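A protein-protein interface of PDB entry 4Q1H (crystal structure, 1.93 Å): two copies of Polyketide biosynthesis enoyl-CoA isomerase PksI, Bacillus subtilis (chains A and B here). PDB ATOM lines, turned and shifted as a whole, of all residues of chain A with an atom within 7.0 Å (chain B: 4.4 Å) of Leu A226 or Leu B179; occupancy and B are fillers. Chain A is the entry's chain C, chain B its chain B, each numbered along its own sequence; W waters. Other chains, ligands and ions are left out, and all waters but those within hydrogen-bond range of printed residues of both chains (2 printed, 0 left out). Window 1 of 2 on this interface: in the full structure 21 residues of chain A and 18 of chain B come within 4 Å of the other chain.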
ATOM      1  N   PRO A 115     -13.953 -18.753 -23.048  1.00  0.00           N
ATOM      2  CA  PRO A 115     -13.039 -19.411 -22.053  1.00  0.00           C
ATOM      3  C   PRO A 115     -11.673 -19.649 -22.619  1.00  0.00           C
ATOM      4  O   PRO A 115     -11.555 -20.072 -23.802  1.00  0.00           O
ATOM      5  CB  PRO A 115     -13.678 -20.762 -21.847  1.00  0.00           C
ATOM      6  CG  PRO A 115     -15.169 -20.433 -21.957  1.00  0.00           C
ATOM      7  CD  PRO A 115     -15.184 -19.545 -23.198  1.00  0.00           C
ATOM      8  N   VAL A 116     -10.654 -19.317 -21.823  1.00  0.00           N
ATOM      9  CA  VAL A 116      -9.274 -19.519 -22.214  1.00  0.00           C
ATOM     10  C   VAL A 116      -8.666 -20.487 -21.216  1.00  0.00           C
ATOM     11  O   VAL A 116      -8.796 -20.314 -20.010  1.00  0.00           O
ATOM     12  CB  VAL A 116      -8.463 -18.189 -22.263  1.00  0.00           C
ATOM     13  CG1 VAL A 116      -6.989 -18.449 -22.646  1.00  0.00           C
ATOM     14  CG2 VAL A 116      -9.138 -17.172 -23.262  1.00  0.00           C
ATOM     15  N   ASP A 136      -9.133 -18.446 -17.735  1.00  0.00           N
ATOM     16  CA  ASP A 136     -10.230 -18.946 -16.918  1.00  0.00           C
ATOM     17  C   ASP A 136      -9.834 -20.270 -16.260  1.00  0.00           C
ATOM     18  O   ASP A 136     -10.383 -20.578 -15.200  1.00  0.00           O
ATOM     19  CB  ASP A 136     -11.463 -19.161 -17.810  1.00  0.00           C
ATOM     20  CG  ASP A 136     -11.792 -17.816 -18.533  1.00  0.00           C
ATOM     21  OD1 ASP A 136     -12.299 -16.915 -17.798  1.00  0.00           O
ATOM     22  OD2 ASP A 136     -11.386 -17.628 -19.706  1.00  0.00           O
ATOM     23  N   ILE A 137      -9.040 -21.089 -16.947  1.00  0.00           N
ATOM     24  CA  ILE A 137      -8.645 -22.428 -16.374  1.00  0.00           C
ATOM     25  C   ILE A 137      -7.115 -22.483 -16.552  1.00  0.00           C
ATOM     26  O   ILE A 137      -6.616 -22.201 -17.663  1.00  0.00           O
ATOM     27  CB  ILE A 137      -9.330 -23.581 -17.144  1.00  0.00           C
ATOM     28  CG1 ILE A 137     -10.884 -23.505 -16.867  1.00  0.00           C
ATOM     29  CG2 ILE A 137      -8.794 -24.927 -16.636  1.00  0.00           C
ATOM     30  CD1 ILE A 137     -11.747 -24.454 -17.687  1.00  0.00           C
ATOM     31  N   GLU A 214     -14.762 -30.664 -24.029  1.00  0.00           N
ATOM     32  CA  GLU A 214     -15.960 -30.620 -23.153  1.00  0.00           C
ATOM     33  C   GLU A 214     -16.608 -29.214 -23.133  1.00  0.00           C
ATOM     34  O   GLU A 214     -17.871 -29.135 -23.142  1.00  0.00           O
ATOM     35  CB  GLU A 214     -15.611 -31.033 -21.739  1.00  0.00           C
ATOM     36  CG  GLU A 214     -15.199 -32.544 -21.775  1.00  0.00           C
ATOM     37  CD  GLU A 214     -14.515 -33.003 -20.492  1.00  0.00           C
ATOM     38  OE1 GLU A 214     -14.432 -32.216 -19.484  1.00  0.00           O
ATOM     39  OE2 GLU A 214     -13.968 -34.132 -20.511  1.00  0.00           O
ATOM     40  N   LEU A 215     -15.795 -28.159 -23.052  1.00  0.00           N
ATOM     41  CA  LEU A 215     -16.383 -26.788 -23.062  1.00  0.00           C
ATOM     42  C   LEU A 215     -17.120 -26.542 -24.376  1.00  0.00           C
ATOM     43  O   LEU A 215     -18.196 -25.909 -24.379  1.00  0.00           O
ATOM     44  CB  LEU A 215     -15.319 -25.718 -22.923  1.00  0.00           C
ATOM     45  CG  LEU A 215     -14.691 -25.694 -21.504  1.00  0.00           C
ATOM     46  CD1 LEU A 215     -13.402 -24.861 -21.640  1.00  0.00           C
ATOM     47  CD2 LEU A 215     -15.620 -24.923 -20.500  1.00  0.00           C
ATOM     48  N   LYS A 218     -20.966 -26.862 -25.113  1.00  0.00           N
ATOM     49  CA  LYS A 218     -21.966 -25.913 -24.595  1.00  0.00           C
ATOM     50  C   LYS A 218     -22.337 -24.951 -25.726  1.00  0.00           C
ATOM     51  O   LYS A 218     -21.483 -24.632 -26.546  1.00  0.00           O
ATOM     52  CB  LYS A 218     -21.363 -25.103 -23.396  1.00  0.00           C
ATOM     53  CG  LYS A 218     -21.485 -25.831 -22.047  1.00  0.00           C
ATOM     54  CD  LYS A 218     -20.607 -27.086 -22.100  1.00  0.00           C
ATOM     55  CE  LYS A 218     -20.209 -27.498 -20.675  1.00  0.00           C
ATOM     56  NZ  LYS A 218     -19.428 -28.807 -20.858  1.00  0.00           N
ATOM     57  N   ARG A 220     -22.391 -21.565 -27.482  1.00  0.00           N
ATOM     58  CA  ARG A 220     -21.472 -20.474 -27.358  1.00  0.00           C
ATOM     59  C   ARG A 220     -22.033 -19.308 -26.511  1.00  0.00           C
ATOM     60  O   ARG A 220     -21.376 -18.742 -25.705  1.00  0.00           O
ATOM     61  CB  ARG A 220     -21.022 -19.961 -28.711  1.00  0.00           C
ATOM     62  CG  ARG A 220     -19.873 -18.976 -28.613  1.00  0.00           C
ATOM     63  CD  ARG A 220     -19.421 -18.471 -29.963  1.00  0.00           C
ATOM     64  NE  ARG A 220     -18.224 -17.677 -29.967  1.00  0.00           N
ATOM     65  CZ  ARG A 220     -18.135 -16.385 -29.736  1.00  0.00           C
ATOM     66  NH1 ARG A 220     -19.173 -15.656 -29.449  1.00  0.00           N
ATOM     67  NH2 ARG A 220     -16.981 -15.812 -29.788  1.00  0.00           N
ATOM     68  N   ASN A 221     -23.291 -19.007 -26.716  1.00  0.00           N
ATOM     69  CA  ASN A 221     -23.885 -17.823 -26.023  1.00  0.00           C
ATOM     70  C   ASN A 221     -23.911 -18.150 -24.521  1.00  0.00           C
ATOM     71  O   ASN A 221     -23.817 -17.226 -23.671  1.00  0.00           O
ATOM     72  CB  ASN A 221     -25.355 -17.573 -26.514  1.00  0.00           C
ATOM     73  CG  ASN A 221     -26.029 -16.462 -25.737  1.00  0.00           C
ATOM     74  OD1 ASN A 221     -25.539 -15.322 -25.705  1.00  0.00           O
ATOM     75  ND2 ASN A 221     -27.152 -16.767 -25.114  1.00  0.00           N
ATOM     76  N   SER A 222     -24.130 -19.408 -24.147  1.00  0.00           N
ATOM     77  CA  SER A 222     -24.096 -19.710 -22.681  1.00  0.00           C
ATOM     78  C   SER A 222     -22.684 -19.518 -22.067  1.00  0.00           C
ATOM     79  O   SER A 222     -22.572 -18.951 -20.958  1.00  0.00           O
ATOM     80  CB  SER A 222     -24.561 -21.122 -22.335  1.00  0.00           C
ATOM     81  OG  SER A 222     -25.851 -21.354 -22.867  1.00  0.00           O
ATOM     82  N   LEU A 223     -21.664 -20.035 -22.760  1.00  0.00           N
ATOM     83  CA  LEU A 223     -20.238 -19.854 -22.329  1.00  0.00           C
ATOM     84  C   LEU A 223     -19.953 -18.351 -22.119  1.00  0.00           C
ATOM     85  O   LEU A 223     -19.291 -17.928 -21.120  1.00  0.00           O
ATOM     86  CB  LEU A 223     -19.246 -20.387 -23.369  1.00  0.00           C
ATOM     87  CG  LEU A 223     -19.263 -21.937 -23.503  1.00  0.00           C
ATOM     88  CD1 LEU A 223     -18.455 -22.476 -24.685  1.00  0.00           C
ATOM     89  CD2 LEU A 223     -18.786 -22.624 -22.218  1.00  0.00           C
ATOM     90  N   VAL A 224     -20.272 -17.559 -23.147  1.00  0.00           N
ATOM     91  CA  VAL A 224     -19.915 -16.144 -23.091  1.00  0.00           C
ATOM     92  C   VAL A 224     -20.691 -15.387 -21.983  1.00  0.00           C
ATOM     93  O   VAL A 224     -20.126 -14.579 -21.220  1.00  0.00           O
ATOM     94  CB  VAL A 224     -20.122 -15.435 -24.517  1.00  0.00           C
ATOM     95  CG1 VAL A 224     -19.972 -13.930 -24.288  1.00  0.00           C
ATOM     96  CG2 VAL A 224     -19.088 -16.043 -25.512  1.00  0.00           C
ATOM     97  N   THR A 225     -21.973 -15.673 -21.877  1.00  0.00           N
ATOM     98  CA  THR A 225     -22.851 -15.010 -20.851  1.00  0.00           C
ATOM     99  C   THR A 225     -22.310 -15.376 -19.464  1.00  0.00           C
ATOM    100  O   THR A 225     -22.228 -14.490 -18.560  1.00  0.00           O
ATOM    101  CB  THR A 225     -24.309 -15.548 -20.953  1.00  0.00           C
ATOM    102  OG1 THR A 225     -24.876 -15.047 -22.211  1.00  0.00           O
ATOM    103  CG2 THR A 225     -25.202 -15.026 -19.832  1.00  0.00           C
ATOM    104  N   LEU A 226     -22.004 -16.654 -19.236  1.00  0.00           N
ATOM    105  CA  LEU A 226     -21.457 -17.002 -17.914  1.00  0.00           C
ATOM    106  C   LEU A 226     -20.041 -16.387 -17.688  1.00  0.00           C
ATOM    107  O   LEU A 226     -19.761 -15.809 -16.632  1.00  0.00           O
ATOM    108  CB  LEU A 226     -21.426 -18.574 -17.803  1.00  0.00           C
ATOM    109  CG  LEU A 226     -20.920 -18.996 -16.425  1.00  0.00           C
ATOM    110  CD1 LEU A 226     -21.776 -18.361 -15.271  1.00  0.00           C
ATOM    111  CD2 LEU A 226     -20.904 -20.564 -16.444  1.00  0.00           C
ATOM    112  N   LYS A 227     -19.124 -16.525 -18.661  1.00  0.00           N
ATOM    113  CA  LYS A 227     -17.787 -15.921 -18.445  1.00  0.00           C
ATOM    114  C   LYS A 227     -17.945 -14.409 -18.170  1.00  0.00           C
ATOM    115  O   LYS A 227     -17.271 -13.863 -17.258  1.00  0.00           O
ATOM    116  CB  LYS A 227     -16.811 -16.166 -19.629  1.00  0.00           C
ATOM    117  CG  LYS A 227     -15.447 -15.410 -19.443  1.00  0.00           C
ATOM    118  CD  LYS A 227     -14.453 -15.713 -20.521  1.00  0.00           C
ATOM    119  CE  LYS A 227     -13.225 -14.863 -20.186  1.00  0.00           C
ATOM    120  NZ  LYS A 227     -12.057 -15.329 -21.038  1.00  0.00           N
ATOM    121  N   ASP A 228     -18.796 -13.723 -18.931  1.00  0.00           N
ATOM    122  CA  ASP A 228     -18.950 -12.228 -18.651  1.00  0.00           C
ATOM    123  C   ASP A 228     -19.315 -11.957 -17.183  1.00  0.00           C
ATOM    124  O   ASP A 228     -18.846 -11.015 -16.552  1.00  0.00           O
ATOM    125  CB  ASP A 228     -20.078 -11.629 -19.521  1.00  0.00           C
ATOM    126  CG  ASP A 228     -19.638 -11.338 -20.949  1.00  0.00           C
ATOM    127  OD1 ASP A 228     -18.403 -11.320 -21.257  1.00  0.00           O
ATOM    128  OD2 ASP A 228     -20.548 -11.088 -21.774  1.00  0.00           O
ATOM    129  N   HIS A 229     -20.206 -12.767 -16.656  1.00  0.00           N
ATOM    130  CA  HIS A 229     -20.610 -12.614 -15.280  1.00  0.00           C
ATOM    131  C   HIS A 229     -19.451 -13.043 -14.307  1.00  0.00           C
ATOM    132  O   HIS A 229     -19.187 -12.324 -13.336  1.00  0.00           O
ATOM    133  CB  HIS A 229     -21.832 -13.490 -15.038  1.00  0.00           C
ATOM    134  CG  HIS A 229     -22.223 -13.580 -13.601  1.00  0.00           C
ATOM    135  ND1 HIS A 229     -22.709 -12.505 -12.900  1.00  0.00           N
ATOM    136  CD2 HIS A 229     -22.197 -14.617 -12.726  1.00  0.00           C
ATOM    137  CE1 HIS A 229     -22.931 -12.859 -11.647  1.00  0.00           C
ATOM    138  NE2 HIS A 229     -22.705 -14.158 -11.537  1.00  0.00           N
ATOM    139  N   LEU A 230     -18.841 -14.211 -14.513  1.00  0.00           N
ATOM    140  CA  LEU A 230     -17.786 -14.677 -13.579  1.00  0.00           C
ATOM    141  C   LEU A 230     -16.617 -13.690 -13.519  1.00  0.00           C
ATOM    142  O   LEU A 230     -16.002 -13.542 -12.454  1.00  0.00           O
ATOM    143  CB  LEU A 230     -17.195 -16.035 -14.000  1.00  0.00           C
ATOM    144  CG  LEU A 230     -18.285 -17.150 -13.890  1.00  0.00           C
ATOM    145  CD1 LEU A 230     -17.808 -18.493 -14.537  1.00  0.00           C
ATOM    146  CD2 LEU A 230     -18.822 -17.257 -12.464  1.00  0.00           C
ATOM    147  N   VAL A 231     -16.277 -13.053 -14.627  1.00  0.00           N
ATOM    148  CA  VAL A 231     -15.080 -12.207 -14.621  1.00  0.00           C
ATOM    149  C   VAL A 231     -15.372 -10.735 -14.561  1.00  0.00           C
ATOM    150  O   VAL A 231     -14.402  -9.943 -14.528  1.00  0.00           O
ATOM    151  CB  VAL A 231     -14.054 -12.495 -15.780  1.00  0.00           C
ATOM    152  CG1 VAL A 231     -13.690 -14.003 -15.773  1.00  0.00           C
ATOM    153  CG2 VAL A 231     -14.623 -12.106 -17.141  1.00  0.00           C
ATOM    154  N   ALA A 232     -16.663 -10.353 -14.505  1.00  0.00           N
ATOM    155  CA  ALA A 232     -17.033  -8.902 -14.396  1.00  0.00           C
ATOM    156  C   ALA A 232     -16.241  -8.204 -13.211  1.00  0.00           C
ATOM    157  O   ALA A 232     -15.647  -7.115 -13.417  1.00  0.00           O
ATOM    158  CB  ALA A 232     -18.574  -8.752 -14.214  1.00  0.00           C
ATOM    159  N   MET B 151     -24.754 -26.085 -16.920  1.00  0.00           N
ATOM    160  CA  MET B 151     -24.304 -25.812 -18.303  1.00  0.00           C
ATOM    161  C   MET B 151     -24.283 -27.008 -19.250  1.00  0.00           C
ATOM    162  O   MET B 151     -24.208 -26.812 -20.447  1.00  0.00           O
ATOM    163  CB  MET B 151     -22.929 -25.102 -18.288  1.00  0.00           C
ATOM    164  CG  MET B 151     -23.071 -23.711 -17.657  1.00  0.00           C
ATOM    165  SD  MET B 151     -23.426 -22.414 -18.907  1.00  0.00           S
ATOM    166  CE  MET B 151     -21.813 -22.353 -19.769  1.00  0.00           C
ATOM    167  N   THR B 156     -27.393 -21.308 -17.731  1.00  0.00           N
ATOM    168  CA  THR B 156     -26.349 -20.767 -16.858  1.00  0.00           C
ATOM    169  C   THR B 156     -26.640 -21.205 -15.398  1.00  0.00           C
ATOM    170  O   THR B 156     -27.785 -21.537 -15.113  1.00  0.00           O
ATOM    171  CB  THR B 156     -26.302 -19.215 -17.006  1.00  0.00           C
ATOM    172  OG1 THR B 156     -27.648 -18.669 -16.943  1.00  0.00           O
ATOM    173  CG2 THR B 156     -25.686 -18.876 -18.384  1.00  0.00           C
ATOM    174  N   PRO B 157     -25.653 -21.190 -14.505  1.00  0.00           N
ATOM    175  CA  PRO B 157     -25.872 -21.806 -13.185  1.00  0.00           C
ATOM    176  C   PRO B 157     -26.825 -20.910 -12.391  1.00  0.00           C
ATOM    177  O   PRO B 157     -26.741 -19.659 -12.486  1.00  0.00           O
ATOM    178  CB  PRO B 157     -24.472 -21.754 -12.535  1.00  0.00           C
ATOM    179  CG  PRO B 157     -23.521 -21.849 -13.731  1.00  0.00           C
ATOM    180  CD  PRO B 157     -24.215 -20.893 -14.700  1.00  0.00           C
ATOM    181  N   THR B 162     -23.276 -19.350  -8.571  1.00  0.00           N
ATOM    182  CA  THR B 162     -22.182 -18.469  -9.004  1.00  0.00           C
ATOM    183  C   THR B 162     -21.624 -17.701  -7.847  1.00  0.00           C
ATOM    184  O   THR B 162     -20.510 -17.102  -7.891  1.00  0.00           O
ATOM    185  CB  THR B 162     -22.562 -17.460 -10.156  1.00  0.00           C
ATOM    186  OG1 THR B 162     -23.583 -16.597  -9.717  1.00  0.00           O
ATOM    187  CG2 THR B 162     -23.139 -18.231 -11.352  1.00  0.00           C
ATOM    188  N   GLN B 175     -14.508 -21.588 -11.484  1.00  0.00           N
ATOM    189  CA  GLN B 175     -14.632 -21.284 -12.916  1.00  0.00           C
ATOM    190  C   GLN B 175     -14.779 -22.600 -13.665  1.00  0.00           C
ATOM    191  O   GLN B 175     -15.623 -22.680 -14.549  1.00  0.00           O
ATOM    192  CB  GLN B 175     -13.393 -20.549 -13.514  1.00  0.00           C
ATOM    193  CG  GLN B 175     -12.953 -19.356 -12.681  1.00  0.00           C
ATOM    194  CD  GLN B 175     -14.065 -18.386 -12.505  1.00  0.00           C
ATOM    195  OE1 GLN B 175     -14.694 -18.260 -11.406  1.00  0.00           O
ATOM    196  NE2 GLN B 175     -14.392 -17.727 -13.581  1.00  0.00           N
ATOM    197  N   GLU B 176     -13.928 -23.598 -13.335  1.00  0.00           N
ATOM    198  CA  GLU B 176     -13.930 -24.824 -14.091  1.00  0.00           C
ATOM    199  C   GLU B 176     -15.230 -25.604 -13.762  1.00  0.00           C
ATOM    200  O   GLU B 176     -15.932 -26.089 -14.632  1.00  0.00           O
ATOM    201  CB  GLU B 176     -12.753 -25.666 -13.518  1.00  0.00           C
ATOM    202  CG  GLU B 176     -12.673 -27.009 -14.107  1.00  0.00           C
ATOM    203  CD  GLU B 176     -11.490 -27.783 -13.437  1.00  0.00           C
ATOM    204  OE1 GLU B 176     -10.419 -27.116 -13.281  1.00  0.00           O
ATOM    205  OE2 GLU B 176     -11.696 -29.003 -13.124  1.00  0.00           O
ATOM    206  N   ILE B 177     -15.583 -25.632 -12.463  1.00  0.00           N
ATOM    207  CA  ILE B 177     -16.841 -26.327 -12.137  1.00  0.00           C
ATOM    208  C   ILE B 177     -18.089 -25.763 -12.851  1.00  0.00           C
ATOM    209  O   ILE B 177     -18.919 -26.535 -13.351  1.00  0.00           O
ATOM    210  CB  ILE B 177     -17.035 -26.299 -10.584  1.00  0.00           C
ATOM    211  CG1 ILE B 177     -16.053 -27.316 -10.014  1.00  0.00           C
ATOM    212  CG2 ILE B 177     -18.494 -26.621 -10.185  1.00  0.00           C
ATOM    213  CD1 ILE B 177     -15.930 -27.045  -8.482  1.00  0.00           C
ATOM    214  N   LEU B 178     -18.197 -24.431 -12.876  1.00  0.00           N
ATOM    215  CA  LEU B 178     -19.443 -23.785 -13.347  1.00  0.00           C
ATOM    216  C   LEU B 178     -19.458 -23.726 -14.889  1.00  0.00           C
ATOM    217  O   LEU B 178     -20.487 -24.022 -15.469  1.00  0.00           O
ATOM    218  CB  LEU B 178     -19.483 -22.318 -12.830  1.00  0.00           C
ATOM    219  CG  LEU B 178     -19.703 -22.357 -11.305  1.00  0.00           C
ATOM    220  CD1 LEU B 178     -19.449 -20.899 -10.789  1.00  0.00           C
ATOM    221  CD2 LEU B 178     -21.121 -22.768 -10.948  1.00  0.00           C
ATOM    222  N   LEU B 179     -18.313 -23.375 -15.510  1.00  0.00           N
ATOM    223  CA  LEU B 179     -18.276 -23.253 -16.982  1.00  0.00           C
ATOM    224  C   LEU B 179     -18.436 -24.634 -17.653  1.00  0.00           C
ATOM    225  O   LEU B 179     -19.134 -24.781 -18.678  1.00  0.00           O
ATOM    226  CB  LEU B 179     -16.890 -22.653 -17.426  1.00  0.00           C
ATOM    227  CG  LEU B 179     -16.754 -21.127 -17.258  1.00  0.00           C
ATOM    228  CD1 LEU B 179     -15.253 -20.874 -17.535  1.00  0.00           C
ATOM    229  CD2 LEU B 179     -17.613 -20.445 -18.342  1.00  0.00           C
ATOM    230  N   ASN B 180     -17.787 -25.638 -17.083  1.00  0.00           N
ATOM    231  CA  ASN B 180     -17.760 -26.933 -17.817  1.00  0.00           C
ATOM    232  C   ASN B 180     -18.760 -27.964 -17.292  1.00  0.00           C
ATOM    233  O   ASN B 180     -19.030 -28.953 -18.018  1.00  0.00           O
ATOM    234  CB  ASN B 180     -16.352 -27.539 -17.799  1.00  0.00           C
ATOM    235  CG  ASN B 180     -16.204 -28.668 -18.801  1.00  0.00           C
ATOM    236  OD1 ASN B 180     -16.662 -28.537 -19.940  1.00  0.00           O
ATOM    237  ND2 ASN B 180     -15.626 -29.818 -18.362  1.00  0.00           N
ATOM    238  N   ALA B 181     -19.395 -27.712 -16.138  1.00  0.00           N
ATOM    239  CA  ALA B 181     -20.435 -28.616 -15.679  1.00  0.00           C
ATOM    240  C   ALA B 181     -19.930 -30.045 -15.553  1.00  0.00           C
ATOM    241  O   ALA B 181     -20.741 -30.954 -15.651  1.00  0.00           O
ATOM    242  CB  ALA B 181     -21.706 -28.560 -16.613  1.00  0.00           C
ATOM    243  N   MET B 248     -28.609 -13.519 -16.308  1.00  0.00           N
ATOM    244  CA  MET B 248     -27.986 -14.582 -17.217  1.00  0.00           C
ATOM    245  C   MET B 248     -29.036 -15.545 -17.737  1.00  0.00           C
ATOM    246  O   MET B 248     -29.037 -15.969 -18.861  1.00  0.00           O
ATOM    247  CB  MET B 248     -26.911 -15.391 -16.478  1.00  0.00           C
ATOM    248  CG  MET B 248     -25.668 -14.540 -16.280  1.00  0.00           C
ATOM    249  SD  MET B 248     -24.371 -15.686 -15.774  1.00  0.00           S
ATOM    250  CE  MET B 248     -24.984 -16.346 -14.219  1.00  0.00           C
HETATM  251  O   HOH W   1     -14.623 -17.564 -16.191  1.00  0.00           O
HETATM  252  O   HOH W   2     -12.258 -17.170 -14.758  1.00  0.00           O
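Of the 12 printed residues of chain B, 8 touch a printed residue of chain A. Hydrophobic or aromatic side chains of chain B that line the printed part of chain A: Met B151, Pro B157, Leu B179 and Met B248. Along chain B the printed residues that touch a printed residue of chain A span positions 151 to 248.
No position is printed for both chains.
Leu B179 touches Leu A215. Met B151 touches Lys A218 (O to CG, 3.3 Å). Lys A218 touches Leu B179. Met B151 touches Ser A222 (CE to O, 3.7 Å). Met B151 touches Leu A226 (CE to CD2, 3.9 Å). CD of Pro B157 touches CD1 of Leu A226, 3.6 Å away. Leu B178 touches Leu A226. SD of Met B248 touches CD1 of Leu A226, 3.8 Å away. SD of Met B248 touches CB of His A229 (3.4 Å). Leu B179 touches Leu A230 (CG to CD1, 3.9 Å).
Val A116 touches none of the printed residues of chain B. Printed residues of chain B within 4 Å of Asp A136: Gln B175. Of the printed residues of chain B, Thr A225 touches Met B248 (3.6 Å). Leu A226 touches just these residues of chain B: Met B151 (3.9 Å), Pro B157 (3.6 Å), Leu B178 (3.6 Å), Leu B179 (3.8 Å) and Met B248 (3.8 Å). Printed residues of chain A within 4 Å of Leu B178: Leu A226 (3.6 Å). Of chain A, only Leu A215 (3.96 Å), Lys A218 (3.5 Å), Leu A226 (3.8 Å) and Leu A230 (3.9 Å) come within 4 Å of Leu B179. Ala B181 touches none of the printed residues of chain A. The nearest residue of chain B that does not touch Leu A226 is Thr B162 (4.2 Å).
OG1 of Thr B162 sits at hydrogen-bond distance from NE2 of His A229 (3.2 Å). ND2 of Asn B180 is in hydrogen-bond range of OE1 of Glu A214, at 2.9 Å. OD1 of Asn B180 lies within hydrogen-bond range of N of Leu A215 (3.3 Å). The backbone carbonyl oxygen (O) of Asn B180 is in hydrogen-bond range of the side-chain amino group (NZ) of Lys A218 (2.9 Å). The backbone carbonyl oxygen of Thr A225 sits close to the side-chain sulfur of Met B248 (3.7 Å).
N of Val A116 lies within hydrogen-bond range of OD2 of Asp A136, at 2.8 Å. The side-chain carboxylate (OD2) of Asp A136 is in salt-bridge range of the side-chain amino group (NZ) of Lys A227, at 2.7 Å. The side-chain amino group of Lys A218 is in hydrogen-bond range of the backbone carbonyl oxygen of Glu A214 (2.8 Å). O of Asn A221 sits at hydrogen-bond distance from OG1 of Thr A225 (2.8 Å).
Water W2 bridges the side-chain amide nitrogen of Gln B175 (2.5 Å) and the side-chain carboxylate of Asp A136 (3.1 Å). Water W1 lies within hydrogen-bond range of the side-chain amide nitrogen of Gln B175 (2.6 Å) and the side-chain carboxylate of Asp A136 (2.9 Å).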
